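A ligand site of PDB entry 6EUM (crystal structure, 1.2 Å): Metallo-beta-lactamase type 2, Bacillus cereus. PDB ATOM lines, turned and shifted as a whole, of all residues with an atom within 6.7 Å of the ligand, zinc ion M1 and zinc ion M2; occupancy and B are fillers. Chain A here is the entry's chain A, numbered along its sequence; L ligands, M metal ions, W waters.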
ATOM      1  N   PHE A  34     -29.422   9.850 -32.124  1.00  0.00           N
ATOM      2  CA  PHE A  34     -30.187  10.179 -30.925  1.00  0.00           C
ATOM      3  C   PHE A  34     -29.946  11.642 -30.569  1.00  0.00           C
ATOM      4  O   PHE A  34     -28.902  11.999 -29.995  1.00  0.00           O
ATOM      5  CB  PHE A  34     -29.803   9.245 -29.784  1.00  0.00           C
ATOM      6  CG  PHE A  34     -30.111   7.811 -30.091  1.00  0.00           C
ATOM      7  CD1 PHE A  34     -31.348   7.275 -29.789  1.00  0.00           C
ATOM      8  CD2 PHE A  34     -29.170   7.016 -30.712  1.00  0.00           C
ATOM      9  CE1 PHE A  34     -31.645   5.964 -30.071  1.00  0.00           C
ATOM     10  CE2 PHE A  34     -29.448   5.713 -30.999  1.00  0.00           C
ATOM     11  CZ  PHE A  34     -30.694   5.176 -30.685  1.00  0.00           C
ATOM     12  N   VAL A  39     -24.545   7.332 -32.540  1.00  0.00           N
ATOM     13  CA  VAL A  39     -24.044   6.432 -31.512  1.00  0.00           C
ATOM     14  C   VAL A  39     -23.864   5.072 -32.185  1.00  0.00           C
ATOM     15  O   VAL A  39     -24.848   4.396 -32.531  1.00  0.00           O
ATOM     16  CB  VAL A  39     -25.041   6.295 -30.365  1.00  0.00           C
ATOM     17  CG1 VAL A  39     -24.472   5.434 -29.302  1.00  0.00           C
ATOM     18  CG2 VAL A  39     -25.423   7.710 -29.829  1.00  0.00           C
ATOM     19  N   SER A  41     -23.010   1.042 -32.630  1.00  0.00           N
ATOM     20  CA  SER A  41     -23.056  -0.181 -31.859  1.00  0.00           C
ATOM     21  C   SER A  41     -22.663  -1.374 -32.725  1.00  0.00           C
ATOM     22  O   SER A  41     -22.954  -1.406 -33.928  1.00  0.00           O
ATOM     23  CB  SER A  41     -24.442  -0.411 -31.260  1.00  0.00           C
ATOM     24  OG  SER A  41     -25.340  -0.645 -32.290  1.00  0.00           O
ATOM     25  N   TRP A  59     -30.409  -1.059 -33.561  1.00  0.00           N
ATOM     26  CA  TRP A  59     -31.225  -0.109 -32.777  1.00  0.00           C
ATOM     27  C   TRP A  59     -32.681  -0.156 -33.107  1.00  0.00           C
ATOM     28  O   TRP A  59     -33.501   0.227 -32.246  1.00  0.00           O
ATOM     29  CB  TRP A  59     -30.720   1.315 -33.090  1.00  0.00           C
ATOM     30  CG  TRP A  59     -29.313   1.590 -32.668  1.00  0.00           C
ATOM     31  CD1 TRP A  59     -28.164   1.593 -33.473  1.00  0.00           C
ATOM     32  CD2 TRP A  59     -28.877   1.974 -31.362  1.00  0.00           C
ATOM     33  NE1 TRP A  59     -27.091   1.964 -32.728  1.00  0.00           N
ATOM     34  CE2 TRP A  59     -27.481   2.176 -31.409  1.00  0.00           C
ATOM     35  CE3 TRP A  59     -29.545   2.148 -30.146  1.00  0.00           C
ATOM     36  CZ2 TRP A  59     -26.754   2.616 -30.291  1.00  0.00           C
ATOM     37  CZ3 TRP A  59     -28.805   2.601 -29.043  1.00  0.00           C
ATOM     38  CH2 TRP A  59     -27.421   2.769 -29.110  1.00  0.00           C
ATOM     39  N   HIS A  86     -28.645  -8.747 -24.563  1.00  0.00           N
ATOM     40  CA  HIS A  86     -29.417  -8.163 -23.452  1.00  0.00           C
ATOM     41  C   HIS A  86     -30.604  -7.443 -24.056  1.00  0.00           C
ATOM     42  O   HIS A  86     -30.733  -7.339 -25.271  1.00  0.00           O
ATOM     43  CB  HIS A  86     -28.643  -7.298 -22.465  1.00  0.00           C
ATOM     44  CG  HIS A  86     -28.082  -6.018 -22.949  1.00  0.00           C
ATOM     45  ND1 HIS A  86     -26.919  -5.916 -23.659  1.00  0.00           N
ATOM     46  CD2 HIS A  86     -28.468  -4.740 -22.706  1.00  0.00           C
ATOM     47  CE1 HIS A  86     -26.657  -4.631 -23.879  1.00  0.00           C
ATOM     48  NE2 HIS A  86     -27.579  -3.889 -23.317  1.00  0.00           N
ATOM     49  N   ALA A  87     -31.488  -6.955 -23.200  1.00  0.00           N
ATOM     50  CA  ALA A  87     -32.786  -6.396 -23.631  1.00  0.00           C
ATOM     51  C   ALA A  87     -32.796  -4.865 -23.747  1.00  0.00           C
ATOM     52  O   ALA A  87     -33.947  -4.325 -23.859  1.00  0.00           O
ATOM     53  CB  ALA A  87     -33.899  -6.840 -22.685  1.00  0.00           C
ATOM     54  N   HIS A  88     -31.743  -4.232 -24.179  1.00  0.00           N
ATOM     55  CA  HIS A  88     -31.733  -2.816 -24.586  1.00  0.00           C
ATOM     56  C   HIS A  88     -31.892  -2.689 -26.131  1.00  0.00           C
ATOM     57  O   HIS A  88     -31.537  -3.591 -26.893  1.00  0.00           O
ATOM     58  CB  HIS A  88     -30.437  -2.115 -24.158  1.00  0.00           C
ATOM     59  CG  HIS A  88     -30.361  -1.795 -22.700  1.00  0.00           C
ATOM     60  ND1 HIS A  88     -29.125  -1.527 -22.104  1.00  0.00           N
ATOM     61  CD2 HIS A  88     -31.317  -1.551 -21.754  1.00  0.00           C
ATOM     62  CE1 HIS A  88     -29.392  -1.119 -20.886  1.00  0.00           C
ATOM     63  NE2 HIS A  88     -30.674  -1.146 -20.629  1.00  0.00           N
ATOM     64  N   ALA A  89     -32.266  -1.493 -26.598  1.00  0.00           N
ATOM     65  CA  ALA A  89     -32.624  -1.258 -27.992  1.00  0.00           C
ATOM     66  C   ALA A  89     -31.471  -1.565 -28.955  1.00  0.00           C
ATOM     67  O   ALA A  89     -31.740  -2.025 -30.062  1.00  0.00           O
ATOM     68  CB  ALA A  89     -33.085   0.185 -28.191  1.00  0.00           C
ATOM     69  N   ASP A  90     -30.215  -1.271 -28.589  1.00  0.00           N
ATOM     70  CA  ASP A  90     -29.108  -1.555 -29.514  1.00  0.00           C
ATOM     71  C   ASP A  90     -29.020  -3.033 -29.840  1.00  0.00           C
ATOM     72  O   ASP A  90     -28.556  -3.378 -30.936  1.00  0.00           O
ATOM     73  CB  ASP A  90     -27.761  -0.981 -28.968  1.00  0.00           C
ATOM     74  CG  ASP A  90     -27.277  -1.516 -27.640  1.00  0.00           C
ATOM     75  OD1 ASP A  90     -28.153  -1.897 -26.806  1.00  0.00           O
ATOM     76  OD2 ASP A  90     -26.023  -1.576 -27.377  1.00  0.00           O
ATOM     77  N   ARG A  91     -29.364  -3.919 -28.916  1.00  0.00           N
ATOM     78  CA  ARG A  91     -29.282  -5.358 -29.086  1.00  0.00           C
ATOM     79  C   ARG A  91     -30.527  -5.934 -29.724  1.00  0.00           C
ATOM     80  O   ARG A  91     -30.459  -6.801 -30.599  1.00  0.00           O
ATOM     81  CB  ARG A  91     -29.116  -5.994 -27.734  1.00  0.00           C
ATOM     82  CG  ARG A  91     -27.980  -5.474 -26.872  1.00  0.00           C
ATOM     83  CD  ARG A  91     -26.577  -5.737 -27.365  1.00  0.00           C
ATOM     84  NE  ARG A  91     -25.985  -4.521 -27.927  1.00  0.00           N
ATOM     85  CZ  ARG A  91     -24.944  -4.485 -28.723  1.00  0.00           C
ATOM     86  NH1 ARG A  91     -24.389  -5.605 -29.121  1.00  0.00           N
ATOM     87  NH2 ARG A  91     -24.420  -3.352 -29.022  1.00  0.00           N
ATOM     88  N   TYR A 120     -41.087  -5.003 -25.964  1.00  0.00           N
ATOM     89  CA  TYR A 120     -40.580  -5.648 -27.161  1.00  0.00           C
ATOM     90  C   TYR A 120     -41.166  -7.040 -27.354  1.00  0.00           C
ATOM     91  O   TYR A 120     -41.523  -7.729 -26.385  1.00  0.00           O
ATOM     92  CB  TYR A 120     -39.046  -5.786 -27.022  1.00  0.00           C
ATOM     93  CG  TYR A 120     -38.268  -4.500 -27.169  1.00  0.00           C
ATOM     94  CD1 TYR A 120     -38.247  -3.818 -28.361  1.00  0.00           C
ATOM     95  CD2 TYR A 120     -37.496  -4.011 -26.111  1.00  0.00           C
ATOM     96  CE1 TYR A 120     -37.554  -2.648 -28.508  1.00  0.00           C
ATOM     97  CE2 TYR A 120     -36.775  -2.805 -26.208  1.00  0.00           C
ATOM     98  CZ  TYR A 120     -36.816  -2.108 -27.410  1.00  0.00           C
ATOM     99  OH  TYR A 120     -36.093  -0.934 -27.508  1.00  0.00           O
ATOM    100  N   HIS A 149     -23.477  -4.473 -16.828  1.00  0.00           N
ATOM    101  CA  HIS A 149     -24.136  -3.401 -17.539  1.00  0.00           C
ATOM    102  C   HIS A 149     -25.662  -3.463 -17.429  1.00  0.00           C
ATOM    103  O   HIS A 149     -26.300  -2.437 -17.247  1.00  0.00           O
ATOM    104  CB  HIS A 149     -23.697  -3.450 -19.005  1.00  0.00           C
ATOM    105  CG  HIS A 149     -24.529  -2.658 -19.931  1.00  0.00           C
ATOM    106  ND1 HIS A 149     -24.519  -1.298 -19.955  1.00  0.00           N
ATOM    107  CD2 HIS A 149     -25.472  -3.045 -20.828  1.00  0.00           C
ATOM    108  CE1 HIS A 149     -25.382  -0.865 -20.865  1.00  0.00           C
ATOM    109  NE2 HIS A 149     -26.027  -1.894 -21.414  1.00  0.00           N
ATOM    110  N   THR A 150     -26.188  -4.689 -17.436  1.00  0.00           N
ATOM    111  CA  THR A 150     -27.569  -4.956 -17.108  1.00  0.00           C
ATOM    112  C   THR A 150     -27.613  -6.228 -16.313  1.00  0.00           C
ATOM    113  O   THR A 150     -26.625  -6.939 -16.146  1.00  0.00           O
ATOM    114  CB  THR A 150     -28.468  -5.153 -18.339  1.00  0.00           C
ATOM    115  OG1 THR A 150     -27.933  -6.213 -19.110  1.00  0.00           O
ATOM    116  CG2 THR A 150     -28.601  -3.904 -19.135  1.00  0.00           C
ATOM    117  N   GLY A 167     -20.002  -7.602 -25.747  1.00  0.00           N
ATOM    118  CA  GLY A 167     -21.219  -6.851 -25.719  1.00  0.00           C
ATOM    119  C   GLY A 167     -21.035  -5.693 -24.764  1.00  0.00           C
ATOM    120  O   GLY A 167     -19.942  -5.192 -24.489  1.00  0.00           O
ATOM    121  N   CSO A 168     -22.143  -5.221 -24.189  1.00  0.00           N
ATOM    122  CA  CSO A 168     -22.095  -3.954 -23.485  1.00  0.00           C
ATOM    123  CB  CSO A 168     -23.381  -3.206 -23.650  1.00  0.00           C
ATOM    124  SG  CSO A 168     -23.935  -3.194 -25.432  1.00  0.00           S
ATOM    125  C   CSO A 168     -21.579  -4.097 -22.048  1.00  0.00           C
ATOM    126  O   CSO A 168     -21.316  -3.077 -21.403  1.00  0.00           O
ATOM    127  N   LEU A 169     -21.343  -5.318 -21.615  1.00  0.00           N
ATOM    128  CA  LEU A 169     -20.560  -5.596 -20.410  1.00  0.00           C
ATOM    129  C   LEU A 169     -19.149  -5.063 -20.506  1.00  0.00           C
ATOM    130  O   LEU A 169     -18.497  -4.816 -19.480  1.00  0.00           O
ATOM    131  CB  LEU A 169     -20.545  -7.140 -20.186  1.00  0.00           C
ATOM    132  CG  LEU A 169     -19.862  -7.644 -18.947  1.00  0.00           C
ATOM    133  CD1 LEU A 169     -20.710  -7.385 -17.700  1.00  0.00           C
ATOM    134  CD2 LEU A 169     -19.579  -9.150 -19.113  1.00  0.00           C
ATOM    135  N   LYS A 171     -16.407  -2.324 -21.981  1.00  0.00           N
ATOM    136  CA  LYS A 171     -16.176  -1.020 -22.540  1.00  0.00           C
ATOM    137  C   LYS A 171     -14.959  -0.993 -23.452  1.00  0.00           C
ATOM    138  O   LYS A 171     -13.928  -1.624 -23.187  1.00  0.00           O
ATOM    139  CB  LYS A 171     -15.998   0.008 -21.429  1.00  0.00           C
ATOM    140  CG  LYS A 171     -17.142   0.007 -20.373  1.00  0.00           C
ATOM    141  CD  LYS A 171     -18.506   0.207 -20.859  1.00  0.00           C
ATOM    142  CE  LYS A 171     -18.804   1.472 -21.405  1.00  0.00           C
ATOM    143  NZ  LYS A 171     -20.300   1.604 -21.755  1.00  0.00           N
ATOM    144  N   LEU A 178     -18.633   4.622 -17.467  1.00  0.00           N
ATOM    145  CA  LEU A 178     -19.440   3.438 -17.652  1.00  0.00           C
ATOM    146  C   LEU A 178     -20.659   3.657 -18.522  1.00  0.00           C
ATOM    147  O   LEU A 178     -21.339   2.657 -18.857  1.00  0.00           O
ATOM    148  CB  LEU A 178     -19.867   2.901 -16.293  1.00  0.00           C
ATOM    149  CG  LEU A 178     -18.693   2.420 -15.446  1.00  0.00           C
ATOM    150  CD1 LEU A 178     -19.250   2.192 -14.023  1.00  0.00           C
ATOM    151  CD2 LEU A 178     -18.114   1.166 -16.047  1.00  0.00           C
ATOM    152  N   GLY A 179     -20.953   4.891 -18.892  1.00  0.00           N
ATOM    153  CA  GLY A 179     -22.117   5.178 -19.681  1.00  0.00           C
ATOM    154  C   GLY A 179     -23.405   5.116 -18.868  1.00  0.00           C
ATOM    155  O   GLY A 179     -23.438   5.460 -17.691  1.00  0.00           O
ATOM    156  N   ASN A 180     -24.485   4.685 -19.489  1.00  0.00           N
ATOM    157  CA  ASN A 180     -25.762   4.692 -18.813  1.00  0.00           C
ATOM    158  C   ASN A 180     -25.811   3.523 -17.838  1.00  0.00           C
ATOM    159  O   ASN A 180     -25.770   2.355 -18.233  1.00  0.00           O
ATOM    160  CB  ASN A 180     -26.874   4.609 -19.851  1.00  0.00           C
ATOM    161  CG  ASN A 180     -28.239   4.825 -19.262  1.00  0.00           C
ATOM    162  OD1 ASN A 180     -28.526   4.278 -18.257  1.00  0.00           O
ATOM    163  ND2 ASN A 180     -29.088   5.604 -19.911  1.00  0.00           N
ATOM    164  N   VAL A 181     -25.918   3.860 -16.559  1.00  0.00           N
ATOM    165  CA  VAL A 181     -25.912   2.874 -15.497  1.00  0.00           C
ATOM    166  C   VAL A 181     -27.281   2.788 -14.806  1.00  0.00           C
ATOM    167  O   VAL A 181     -27.411   2.084 -13.766  1.00  0.00           O
ATOM    168  CB  VAL A 181     -24.788   3.133 -14.492  1.00  0.00           C
ATOM    169  CG1 VAL A 181     -23.434   2.940 -15.150  1.00  0.00           C
ATOM    170  CG2 VAL A 181     -24.908   4.595 -13.918  1.00  0.00           C
ATOM    171  N   ALA A 182     -28.324   3.254 -15.461  1.00  0.00           N
ATOM    172  CA  ALA A 182     -29.643   3.134 -14.858  1.00  0.00           C
ATOM    173  C   ALA A 182     -30.034   1.704 -14.584  1.00  0.00           C
ATOM    174  O   ALA A 182     -30.667   1.415 -13.555  1.00  0.00           O
ATOM    175  CB  ALA A 182     -30.700   3.767 -15.750  1.00  0.00           C
ATOM    176  N   ASP A 183     -29.680   0.772 -15.462  1.00  0.00           N
ATOM    177  CA  ASP A 183     -30.022  -0.609 -15.343  1.00  0.00           C
ATOM    178  C   ASP A 183     -28.851  -1.463 -14.917  1.00  0.00           C
ATOM    179  O   ASP A 183     -28.961  -2.701 -14.943  1.00  0.00           O
ATOM    180  CB  ASP A 183     -30.572  -1.108 -16.678  1.00  0.00           C
ATOM    181  CG  ASP A 183     -31.845  -0.393 -17.116  1.00  0.00           C
ATOM    182  OD1 ASP A 183     -32.649  -0.029 -16.271  1.00  0.00           O
ATOM    183  OD2 ASP A 183     -32.034  -0.253 -18.348  1.00  0.00           O
ATOM    184  N   GLY A 209     -19.480  -3.836 -26.978  1.00  0.00           N
ATOM    185  CA  GLY A 209     -20.767  -3.449 -27.526  1.00  0.00           C
ATOM    186  C   GLY A 209     -20.722  -2.183 -28.383  1.00  0.00           C
ATOM    187  O   GLY A 209     -21.520  -2.005 -29.305  1.00  0.00           O
ATOM    188  N   HIS A 210     -19.819  -1.274 -28.038  1.00  0.00           N
ATOM    189  CA  HIS A 210     -19.628  -0.002 -28.699  1.00  0.00           C
ATOM    190  C   HIS A 210     -18.118   0.231 -28.775  1.00  0.00           C
ATOM    191  O   HIS A 210     -17.429   0.058 -27.783  1.00  0.00           O
ATOM    192  CB  HIS A 210     -20.356   1.167 -27.915  1.00  0.00           C
ATOM    193  CG  HIS A 210     -21.812   0.827 -27.612  1.00  0.00           C
ATOM    194  ND1 HIS A 210     -22.862   1.067 -28.469  1.00  0.00           N
ATOM    195  CD2 HIS A 210     -22.380   0.194 -26.547  1.00  0.00           C
ATOM    196  CE1 HIS A 210     -23.981   0.603 -27.925  1.00  0.00           C
ATOM    197  NE2 HIS A 210     -23.726   0.069 -26.758  1.00  0.00           N
HETATM  198  C1  LIG L   1     -29.067   1.972 -22.127  1.00  0.00           C
HETATM  199  C2  LIG L   1     -30.443   2.000 -22.183  1.00  0.00           C
HETATM  200  C3  LIG L   1     -31.051   2.028 -23.431  1.00  0.00           C
HETATM  201  C4  LIG L   1     -30.263   2.065 -24.564  1.00  0.00           C
HETATM  202  C5  LIG L   1     -28.893   2.064 -24.484  1.00  0.00           C
HETATM  203  C6  LIG L   1     -24.574   0.889 -23.407  1.00  0.00           C
HETATM  204  O1  LIG L   1     -23.974  -0.146 -23.855  1.00  0.00           O
HETATM  205  C7  LIG L   1     -26.040   0.918 -23.644  1.00  0.00           C
HETATM  206  C8  LIG L   1     -26.772   1.920 -23.102  1.00  0.00           C
HETATM  207  C9  LIG L   1     -28.234   2.008 -23.253  1.00  0.00           C
HETATM  208  F1  LIG L   1     -28.466   1.886 -20.914  1.00  0.00           F
HETATM  209  F2  LIG L   1     -28.182   2.214 -25.613  1.00  0.00           F
HETATM  210  F3  LIG L   1     -30.841   2.113 -25.789  1.00  0.00           F
HETATM  211  O2  LIG L   1     -23.999   1.719 -22.729  1.00  0.00           O
HETATM  212  S1  LIG L   1     -26.822  -0.413 -24.594  1.00  0.00           S
HETATM  213 ZN    ZN M   1     -24.947  -1.176 -25.677  1.00  0.00          ZN
HETATM  214 ZN    ZN M   2     -27.380  -1.919 -22.890  1.00  0.00          ZN
HETATM  215  O   HOH W   1     -21.388  -0.638 -22.908  1.00  0.00           O
HETATM  216  O   HOH W   2     -24.337   4.265 -22.161  1.00  0.00           O
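Water W2 bridges an oxygen (O2) of the ligand (2.6 Å) and the backbone NH (N) of Asn 180 (2.7 Å). Water W1 lies within hydrogen-bond range of the side-chain amino group (NZ) of Lys 171 (2.7 Å) and O of CSO 168 (2.9 Å).
Within 4 Å of zinc ion M1: Asp 90, CSO 168 and His 210.
The side-chain carboxylate (OD2) of Asp 90 binds zinc ion M1, 2.1 Å away. A ring nitrogen (NE2) of His 210 is bound to zinc ion M1 (2.1 Å). Zinc ion M1 is bound by SG of CSO 168, 2.3 Å away. Zinc ion M1 is bound by S1 of the ligand, at 2.3 Å. Zinc ion M1 is bound by an oxygen (O1) of the ligand (2.3 Å). Zinc ion M1 has five donor atoms within binding distance.
Zinc ion M2 is bound by ND1 of His 88 (2.0 Å), NE2 of His 149 (2.0 Å), NE2 of His 86 (2.0 Å) and S1 of the ligand (2.3 Å).
NZ of Lys 171 lies within salt-bridge range of O2 of the ligand, 3.8 Å away.
Of the 25 residues printed, 4 come within 4 Å of zinc ion M2.
Trp 59 touches the ligand. Ala 89 touches the ligand. CB of Asn 180 touches F1 of the ligand (3.3 Å). Within 4 Å of the ligand: Trp 59, His 86, His 88, Ala 89, Asp 90, His 149, CSO 168, Lys 171, Asn 180 and His 210.
A ring nitrogen (NE2) of His 88 lies within hydrogen-bond range of the side-chain carboxylate (OD2) of Asp 183 (2.8 Å). The guanidinium group of Arg 91 lies within salt-bridge range of the side-chain carboxylate of Asp 90, at 3.6 Å. The guanidinium group (NE) of Arg 91 lies close to SG of CSO 168, at 3.5 Å. The side-chain amide oxygen (OD1) of Asn 180 lies within hydrogen-bond range of the backbone NH (N) of Ala 182 (3.0 Å). The indole nitrogen (NE1) of Trp 59 sits at hydrogen-bond distance from the side-chain hydroxyl (OG) of Ser 41, at 3.2 Å. The backbone carbonyl oxygen of Val 39 sits at hydrogen-bond distance from the indole nitrogen of Trp 59 (3.3 Å). The side-chain amino group (NZ) of Lys 171 is in hydrogen-bond range of the backbone carbonyl oxygen (O) of Leu 178 (3.3 Å).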
